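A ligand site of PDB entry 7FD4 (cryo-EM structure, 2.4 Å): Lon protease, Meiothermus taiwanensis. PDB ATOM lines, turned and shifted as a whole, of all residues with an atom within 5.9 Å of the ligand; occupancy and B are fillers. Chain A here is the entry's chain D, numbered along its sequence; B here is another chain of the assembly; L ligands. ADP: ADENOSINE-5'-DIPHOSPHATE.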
ATOM      1  N   ASP A 318      31.871 -10.623   7.918  1.00  0.00           N
ATOM      2  CA  ASP A 318      30.480 -10.502   8.307  1.00  0.00           C
ATOM      3  C   ASP A 318      30.225  -9.252   9.145  1.00  0.00           C
ATOM      4  O   ASP A 318      29.063  -8.871   9.326  1.00  0.00           O
ATOM      5  CB  ASP A 318      30.049 -11.752   9.101  1.00  0.00           C
ATOM      6  CG  ASP A 318      28.555 -12.004   9.063  1.00  0.00           C
ATOM      7  OD1 ASP A 318      27.835 -11.240   8.381  1.00  0.00           O
ATOM      8  OD2 ASP A 318      28.101 -12.979   9.697  1.00  0.00           O
ATOM      9  N   HIS A 319      31.277  -8.610   9.641  1.00  0.00           N
ATOM     10  CA  HIS A 319      31.141  -7.396  10.417  1.00  0.00           C
ATOM     11  C   HIS A 319      32.301  -6.463  10.091  1.00  0.00           C
ATOM     12  O   HIS A 319      33.297  -6.868   9.492  1.00  0.00           O
ATOM     13  CB  HIS A 319      31.091  -7.683  11.910  1.00  0.00           C
ATOM     14  CG  HIS A 319      29.817  -8.326  12.351  1.00  0.00           C
ATOM     15  ND1 HIS A 319      29.608  -9.687  12.295  1.00  0.00           N
ATOM     16  CD2 HIS A 319      28.689  -7.799  12.867  1.00  0.00           C
ATOM     17  CE1 HIS A 319      28.403  -9.969  12.746  1.00  0.00           C
ATOM     18  NE2 HIS A 319      27.818  -8.836  13.103  1.00  0.00           N
ATOM     19  N   TYR A 320      32.135  -5.211  10.484  1.00  0.00           N
ATOM     20  CA  TYR A 320      33.009  -4.116  10.122  1.00  0.00           C
ATOM     21  C   TYR A 320      33.451  -3.407  11.398  1.00  0.00           C
ATOM     22  O   TYR A 320      32.614  -3.076  12.230  1.00  0.00           O
ATOM     23  CB  TYR A 320      32.289  -3.126   9.207  1.00  0.00           C
ATOM     24  CG  TYR A 320      33.124  -1.969   8.765  1.00  0.00           C
ATOM     25  CD1 TYR A 320      34.024  -2.091   7.731  1.00  0.00           C
ATOM     26  CD2 TYR A 320      33.017  -0.739   9.400  1.00  0.00           C
ATOM     27  CE1 TYR A 320      34.794  -1.027   7.323  1.00  0.00           C
ATOM     28  CE2 TYR A 320      33.784   0.325   9.006  1.00  0.00           C
ATOM     29  CZ  TYR A 320      34.668   0.177   7.963  1.00  0.00           C
ATOM     30  OH  TYR A 320      35.430   1.244   7.560  1.00  0.00           O
ATOM     31  N   GLY A 321      34.746  -3.163  11.518  1.00  0.00           N
ATOM     32  CA  GLY A 321      35.253  -2.608  12.754  1.00  0.00           C
ATOM     33  C   GLY A 321      35.138  -3.642  13.853  1.00  0.00           C
ATOM     34  O   GLY A 321      35.446  -4.819  13.636  1.00  0.00           O
ATOM     35  N   LEU A 322      34.642  -3.205  15.018  1.00  0.00           N
ATOM     36  CA  LEU A 322      34.439  -4.033  16.207  1.00  0.00           C
ATOM     37  C   LEU A 322      35.738  -4.743  16.613  1.00  0.00           C
ATOM     38  O   LEU A 322      35.818  -5.975  16.598  1.00  0.00           O
ATOM     39  CB  LEU A 322      33.310  -5.045  16.006  1.00  0.00           C
ATOM     40  CG  LEU A 322      31.917  -4.478  15.812  1.00  0.00           C
ATOM     41  CD1 LEU A 322      30.940  -5.603  15.546  1.00  0.00           C
ATOM     42  CD2 LEU A 322      31.515  -3.713  17.024  1.00  0.00           C
ATOM     43  N   PRO A 356      24.849   0.194  22.707  1.00  0.00           N
ATOM     44  CA  PRO A 356      23.544   0.740  22.391  1.00  0.00           C
ATOM     45  C   PRO A 356      22.805  -0.197  21.449  1.00  0.00           C
ATOM     46  O   PRO A 356      23.442  -0.992  20.757  1.00  0.00           O
ATOM     47  CB  PRO A 356      23.881   2.077  21.728  1.00  0.00           C
ATOM     48  CG  PRO A 356      25.185   1.859  21.128  1.00  0.00           C
ATOM     49  CD  PRO A 356      25.931   0.955  22.051  1.00  0.00           C
ATOM     50  N   PRO A 357      21.472  -0.136  21.418  1.00  0.00           N
ATOM     51  CA  PRO A 357      20.730  -1.075  20.571  1.00  0.00           C
ATOM     52  C   PRO A 357      20.891  -0.780  19.090  1.00  0.00           C
ATOM     53  O   PRO A 357      20.793   0.359  18.647  1.00  0.00           O
ATOM     54  CB  PRO A 357      19.278  -0.878  21.012  1.00  0.00           C
ATOM     55  CG  PRO A 357      19.245   0.476  21.571  1.00  0.00           C
ATOM     56  CD  PRO A 357      20.570   0.698  22.218  1.00  0.00           C
ATOM     57  N   GLY A 358      21.153  -1.830  18.335  1.00  0.00           N
ATOM     58  CA  GLY A 358      21.340  -1.721  16.909  1.00  0.00           C
ATOM     59  C   GLY A 358      22.710  -2.100  16.429  1.00  0.00           C
ATOM     60  O   GLY A 358      22.865  -2.419  15.246  1.00  0.00           O
ATOM     61  N   VAL A 359      23.712  -2.046  17.277  1.00  0.00           N
ATOM     62  CA  VAL A 359      25.036  -2.496  16.885  1.00  0.00           C
ATOM     63  C   VAL A 359      25.026  -4.017  16.902  1.00  0.00           C
ATOM     64  O   VAL A 359      24.348  -4.627  17.728  1.00  0.00           O
ATOM     65  CB  VAL A 359      26.107  -1.922  17.820  1.00  0.00           C
ATOM     66  CG1 VAL A 359      27.443  -2.110  17.233  1.00  0.00           C
ATOM     67  CG2 VAL A 359      25.830  -0.469  18.116  1.00  0.00           C
ATOM     68  N   GLY A 360      25.785  -4.639  16.025  1.00  0.00           N
ATOM     69  CA  GLY A 360      25.617  -6.063  15.778  1.00  0.00           C
ATOM     70  C   GLY A 360      26.131  -6.954  16.878  1.00  0.00           C
ATOM     71  O   GLY A 360      27.168  -7.599  16.719  1.00  0.00           O
ATOM     72  N   LYS A 361      25.427  -7.014  18.014  1.00  0.00           N
ATOM     73  CA  LYS A 361      25.853  -7.880  19.097  1.00  0.00           C
ATOM     74  C   LYS A 361      25.457  -9.329  18.840  1.00  0.00           C
ATOM     75  O   LYS A 361      26.306 -10.220  18.906  1.00  0.00           O
ATOM     76  CB  LYS A 361      25.258  -7.386  20.424  1.00  0.00           C
ATOM     77  CG  LYS A 361      25.730  -6.016  20.806  1.00  0.00           C
ATOM     78  CD  LYS A 361      25.299  -5.647  22.210  1.00  0.00           C
ATOM     79  CE  LYS A 361      23.826  -5.362  22.313  1.00  0.00           C
ATOM     80  NZ  LYS A 361      23.471  -4.078  21.673  1.00  0.00           N
ATOM     81  N   THR A 362      24.179  -9.562  18.527  1.00  0.00           N
ATOM     82  CA  THR A 362      23.669 -10.924  18.331  1.00  0.00           C
ATOM     83  C   THR A 362      24.275 -11.588  17.105  1.00  0.00           C
ATOM     84  O   THR A 362      24.704 -12.760  17.150  1.00  0.00           O
ATOM     85  CB  THR A 362      22.153 -10.851  18.203  1.00  0.00           C
ATOM     86  OG1 THR A 362      21.591 -10.246  19.377  1.00  0.00           O
ATOM     87  CG2 THR A 362      21.558 -12.221  18.016  1.00  0.00           C
ATOM     88  N   SER A 363      24.347 -10.850  15.998  1.00  0.00           N
ATOM     89  CA  SER A 363      24.957 -11.365  14.786  1.00  0.00           C
ATOM     90  C   SER A 363      26.441 -11.611  14.968  1.00  0.00           C
ATOM     91  O   SER A 363      27.010 -12.466  14.285  1.00  0.00           O
ATOM     92  CB  SER A 363      24.716 -10.388  13.632  1.00  0.00           C
ATOM     93  OG  SER A 363      25.377  -9.165  13.873  1.00  0.00           O
ATOM     94  N   LEU A 364      27.068 -10.898  15.888  1.00  0.00           N
ATOM     95  CA  LEU A 364      28.454 -11.218  16.197  1.00  0.00           C
ATOM     96  C   LEU A 364      28.543 -12.528  16.962  1.00  0.00           C
ATOM     97  O   LEU A 364      29.526 -13.248  16.802  1.00  0.00           O
ATOM     98  CB  LEU A 364      29.109 -10.090  16.989  1.00  0.00           C
ATOM     99  CG  LEU A 364      30.618 -10.118  17.120  1.00  0.00           C
ATOM    100  CD1 LEU A 364      31.248 -10.138  15.759  1.00  0.00           C
ATOM    101  CD2 LEU A 364      31.031  -8.877  17.839  1.00  0.00           C
ATOM    102  N   ASN A 472      22.468  -3.688  27.384  1.00  0.00           N
ATOM    103  CA  ASN A 472      22.547  -2.288  26.983  1.00  0.00           C
ATOM    104  C   ASN A 472      23.162  -1.392  28.028  1.00  0.00           C
ATOM    105  O   ASN A 472      23.943  -0.510  27.706  1.00  0.00           O
ATOM    106  CB  ASN A 472      21.158  -1.760  26.625  1.00  0.00           C
ATOM    107  CG  ASN A 472      20.628  -2.335  25.327  1.00  0.00           C
ATOM    108  OD1 ASN A 472      21.361  -2.478  24.355  1.00  0.00           O
ATOM    109  ND2 ASN A 472      19.346  -2.654  25.308  1.00  0.00           N
ATOM    110  N   TYR A 493      28.548   4.043  16.153  1.00  0.00           N
ATOM    111  CA  TYR A 493      29.182   4.375  14.881  1.00  0.00           C
ATOM    112  C   TYR A 493      29.078   5.847  14.540  1.00  0.00           C
ATOM    113  O   TYR A 493      28.117   6.528  14.912  1.00  0.00           O
ATOM    114  CB  TYR A 493      28.547   3.565  13.753  1.00  0.00           C
ATOM    115  CG  TYR A 493      28.696   2.091  13.952  1.00  0.00           C
ATOM    116  CD1 TYR A 493      29.925   1.486  13.816  1.00  0.00           C
ATOM    117  CD2 TYR A 493      27.602   1.306  14.235  1.00  0.00           C
ATOM    118  CE1 TYR A 493      30.068   0.155  13.998  1.00  0.00           C
ATOM    119  CE2 TYR A 493      27.737  -0.032  14.408  1.00  0.00           C
ATOM    120  CZ  TYR A 493      28.974  -0.609  14.287  1.00  0.00           C
ATOM    121  OH  TYR A 493      29.125  -1.953  14.449  1.00  0.00           O
ATOM    122  N   ILE A 501      29.544   0.874   6.161  1.00  0.00           N
ATOM    123  CA  ILE A 501      28.755  -0.317   6.441  1.00  0.00           C
ATOM    124  C   ILE A 501      27.628  -0.454   5.428  1.00  0.00           C
ATOM    125  O   ILE A 501      27.422  -1.537   4.860  1.00  0.00           O
ATOM    126  CB  ILE A 501      28.199  -0.287   7.870  1.00  0.00           C
ATOM    127  CG1 ILE A 501      29.310  -0.511   8.878  1.00  0.00           C
ATOM    128  CG2 ILE A 501      27.155  -1.339   8.079  1.00  0.00           C
ATOM    129  CD1 ILE A 501      28.884  -0.175  10.271  1.00  0.00           C
ATOM    130  N   TYR A 505      28.065  -3.788   3.200  1.00  0.00           N
ATOM    131  CA  TYR A 505      27.356  -4.916   3.780  1.00  0.00           C
ATOM    132  C   TYR A 505      25.847  -4.844   3.625  1.00  0.00           C
ATOM    133  O   TYR A 505      25.232  -5.818   3.190  1.00  0.00           O
ATOM    134  CB  TYR A 505      27.725  -5.039   5.264  1.00  0.00           C
ATOM    135  CG  TYR A 505      29.166  -5.389   5.500  1.00  0.00           C
ATOM    136  CD1 TYR A 505      29.607  -6.689   5.388  1.00  0.00           C
ATOM    137  CD2 TYR A 505      30.084  -4.416   5.863  1.00  0.00           C
ATOM    138  CE1 TYR A 505      30.923  -7.009   5.607  1.00  0.00           C
ATOM    139  CE2 TYR A 505      31.396  -4.724   6.087  1.00  0.00           C
ATOM    140  CZ  TYR A 505      31.811  -6.024   5.954  1.00  0.00           C
ATOM    141  OH  TYR A 505      33.116  -6.350   6.177  1.00  0.00           O
ATOM    142  N   LEU A 506      25.237  -3.710   3.960  1.00  0.00           N
ATOM    143  CA  LEU A 506      23.783  -3.673   4.105  1.00  0.00           C
ATOM    144  C   LEU A 506      23.073  -3.632   2.761  1.00  0.00           C
ATOM    145  O   LEU A 506      22.097  -4.360   2.551  1.00  0.00           O
ATOM    146  CB  LEU A 506      23.368  -2.466   4.936  1.00  0.00           C
ATOM    147  CG  LEU A 506      23.789  -2.458   6.403  1.00  0.00           C
ATOM    148  CD1 LEU A 506      23.344  -1.176   7.025  1.00  0.00           C
ATOM    149  CD2 LEU A 506      23.182  -3.633   7.113  1.00  0.00           C
ATOM    150  N   LYS A 509      23.103  -6.978   0.412  1.00  0.00           N
ATOM    151  CA  LYS A 509      22.221  -7.970   0.992  1.00  0.00           C
ATOM    152  C   LYS A 509      20.763  -7.634   0.738  1.00  0.00           C
ATOM    153  O   LYS A 509      19.978  -8.521   0.395  1.00  0.00           O
ATOM    154  CB  LYS A 509      22.487  -8.063   2.493  1.00  0.00           C
ATOM    155  CG  LYS A 509      21.651  -9.079   3.217  1.00  0.00           C
ATOM    156  CD  LYS A 509      22.077  -9.149   4.661  1.00  0.00           C
ATOM    157  CE  LYS A 509      21.652  -7.891   5.406  1.00  0.00           C
ATOM    158  NZ  LYS A 509      21.964  -7.957   6.865  1.00  0.00           N
ATOM    159  N   VAL A 540      22.468   0.363  13.259  1.00  0.00           N
ATOM    160  CA  VAL A 540      22.105   0.318  11.845  1.00  0.00           C
ATOM    161  C   VAL A 540      20.864  -0.526  11.585  1.00  0.00           C
ATOM    162  O   VAL A 540      20.721  -1.084  10.490  1.00  0.00           O
ATOM    163  CB  VAL A 540      23.287  -0.197  11.000  1.00  0.00           C
ATOM    164  CG1 VAL A 540      24.380   0.830  10.921  1.00  0.00           C
ATOM    165  CG2 VAL A 540      23.828  -1.458  11.603  1.00  0.00           C
ATOM    166  N   ARG A 541      19.969  -0.642  12.554  1.00  0.00           N
ATOM    167  CA  ARG A 541      18.684  -1.295  12.286  1.00  0.00           C
ATOM    168  C   ARG A 541      17.821  -0.451  11.352  1.00  0.00           C
ATOM    169  O   ARG A 541      17.297  -0.954  10.349  1.00  0.00           O
ATOM    170  CB  ARG A 541      17.910  -1.559  13.570  1.00  0.00           C
ATOM    171  CG  ARG A 541      18.394  -2.709  14.408  1.00  0.00           C
ATOM    172  CD  ARG A 541      17.521  -2.822  15.645  1.00  0.00           C
ATOM    173  NE  ARG A 541      17.965  -3.862  16.568  1.00  0.00           N
ATOM    174  CZ  ARG A 541      17.457  -4.048  17.775  1.00  0.00           C
ATOM    175  NH1 ARG A 541      16.484  -3.257  18.218  1.00  0.00           N
ATOM    176  NH2 ARG A 541      17.915  -5.012  18.559  1.00  0.00           N
ATOM    177  N   GLU A 544      19.130  -0.184   7.747  1.00  0.00           N
ATOM    178  CA  GLU A 544      18.863  -1.408   7.012  1.00  0.00           C
ATOM    179  C   GLU A 544      17.411  -1.489   6.588  1.00  0.00           C
ATOM    180  O   GLU A 544      17.117  -1.886   5.453  1.00  0.00           O
ATOM    181  CB  GLU A 544      19.227  -2.607   7.867  1.00  0.00           C
ATOM    182  CG  GLU A 544      19.156  -3.922   7.142  1.00  0.00           C
ATOM    183  CD  GLU A 544      19.512  -5.087   8.022  1.00  0.00           C
ATOM    184  OE1 GLU A 544      19.755  -4.866   9.221  1.00  0.00           O
ATOM    185  OE2 GLU A 544      19.566  -6.224   7.521  1.00  0.00           O
ATOM    186  N   ASP B 483      12.322  -9.070  15.792  1.00  0.00           N
ATOM    187  CA  ASP B 483      13.548  -9.108  15.001  1.00  0.00           C
ATOM    188  C   ASP B 483      13.249  -9.502  13.566  1.00  0.00           C
ATOM    189  O   ASP B 483      13.849  -8.964  12.623  1.00  0.00           O
ATOM    190  CB  ASP B 483      14.542 -10.080  15.632  1.00  0.00           C
ATOM    191  CG  ASP B 483      15.963  -9.926  15.089  1.00  0.00           C
ATOM    192  OD1 ASP B 483      16.213  -9.043  14.251  1.00  0.00           O
ATOM    193  OD2 ASP B 483      16.833 -10.730  15.505  1.00  0.00           O
HETATM  194  PB  ADP L   1      21.209  -5.744  18.310  1.00  0.00           P
HETATM  195  O1B ADP L   1      22.046  -5.034  19.325  1.00  0.00           O
HETATM  196  O2B ADP L   1      20.458  -4.838  17.378  1.00  0.00           O
HETATM  197  O3B ADP L   1      20.376  -6.833  18.908  1.00  0.00           O
HETATM  198  PA  ADP L   1      21.739  -7.242  15.985  1.00  0.00           P
HETATM  199  O1A ADP L   1      22.927  -7.908  15.355  1.00  0.00           O
HETATM  200  O2A ADP L   1      20.509  -8.049  16.302  1.00  0.00           O
HETATM  201  O3A ADP L   1      22.227  -6.488  17.307  1.00  0.00           O
HETATM  202  O5' ADP L   1      21.281  -6.127  14.938  1.00  0.00           O
HETATM  203  C5' ADP L   1      22.271  -5.474  14.163  1.00  0.00           C
HETATM  204  C4' ADP L   1      21.980  -5.588  12.669  1.00  0.00           C
HETATM  205  O4' ADP L   1      22.987  -4.890  11.955  1.00  0.00           O
HETATM  206  C3' ADP L   1      22.073  -7.036  12.240  1.00  0.00           C
HETATM  207  O3' ADP L   1      20.902  -7.371  11.492  1.00  0.00           O
HETATM  208  C2' ADP L   1      23.261  -7.129  11.327  1.00  0.00           C
HETATM  209  O2' ADP L   1      22.943  -7.894  10.179  1.00  0.00           O
HETATM  210  C1' ADP L   1      23.482  -5.710  10.901  1.00  0.00           C
HETATM  211  N9  ADP L   1      24.913  -5.473  10.596  1.00  0.00           N
HETATM  212  C8  ADP L   1      25.511  -5.867   9.468  1.00  0.00           C
HETATM  213  N7  ADP L   1      26.815  -5.502   9.452  1.00  0.00           N
HETATM  214  C5  ADP L   1      27.047  -4.853  10.593  1.00  0.00           C
HETATM  215  C6  ADP L   1      28.207  -4.227  11.190  1.00  0.00           C
HETATM  216  N6  ADP L   1      29.370  -4.212  10.540  1.00  0.00           N
HETATM  217  N1  ADP L   1      28.074  -3.658  12.391  1.00  0.00           N
HETATM  218  C2  ADP L   1      26.890  -3.675  13.028  1.00  0.00           C
HETATM  219  N3  ADP L   1      25.787  -4.242  12.544  1.00  0.00           N
HETATM  220  C4  ADP L   1      25.799  -4.838  11.343  1.00  0.00           C
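N1 of the ligand sits at hydrogen-bond distance from OH of Tyr 493 (2.9 Å). An oxygen (O2B) of the ligand lies within salt-bridge range of the guanidinium group (NE) of Arg 541 (2.8 Å). The backbone NH (N) of Gly 358 is in hydrogen-bond range of an oxygen (O2B) of the ligand. The side-chain amino group (NZ) of Lys 361 lies within salt-bridge range of an oxygen (O1B) of the ligand (2.9 Å). An oxygen (O1A) of the ligand is in hydrogen-bond range of the backbone NH (N) of Ser 363 (3.3 Å). The backbone NH (N) of Lys 361 sits at hydrogen-bond distance from an oxygen (O3A) of the ligand (3.3 Å). O2' of the ligand is in hydrogen-bond range of NZ of Lys 509 (3.5 Å). O of Val 359 lies close to O1B of the ligand. An oxygen (O1A) of the ligand sits at hydrogen-bond distance from the side-chain hydroxyl (OG) of Ser 363, 3.1 Å away.
O of Pro 356 sits at hydrogen-bond distance from NZ of Lys 361 (3.2 Å). O of His 319 lies within hydrogen-bond range of OH of Tyr 505 (3.4 Å). O of Gly 358 lies within hydrogen-bond range of N of Val 540 (3.4 Å). NZ of Lys 509 lies within salt-bridge range of OE2 of Glu 544 (3.0 Å). The backbone NH of Leu 506 lies within hydrogen-bond range of the backbone carbonyl oxygen of Ile 501, at 3.2 Å. A ring nitrogen (NE2) of His 319 lies within hydrogen-bond range of the side-chain hydroxyl (OG) of Ser 363, at 2.6 Å.
The backbone NH of Tyr 320 sits close to a nitrogen (N6) of the ligand, 2.9 Å away. His 319 touches the ligand (CA to N6, 3.6 Å). CA of Gly 360 touches O1A of the ligand, 3.3 Å away. Thr 362 touches the ligand (OG1 to O3B, 3.7 Å). CD2 of Leu 506 touches C8 of the ligand (3.995 Å). Val 540 touches the ligand (CG2 to N3, 3.5 Å). Glu 544 touches the ligand (OE1 to O3', 3.6 Å). Hydrophobic or aromatic side chains within 4 Å of the ligand: His 319, Tyr 320, Tyr 493, Leu 506 and Val 540. Of the 24 residues printed, 14 come within 4 Å of the ligand.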
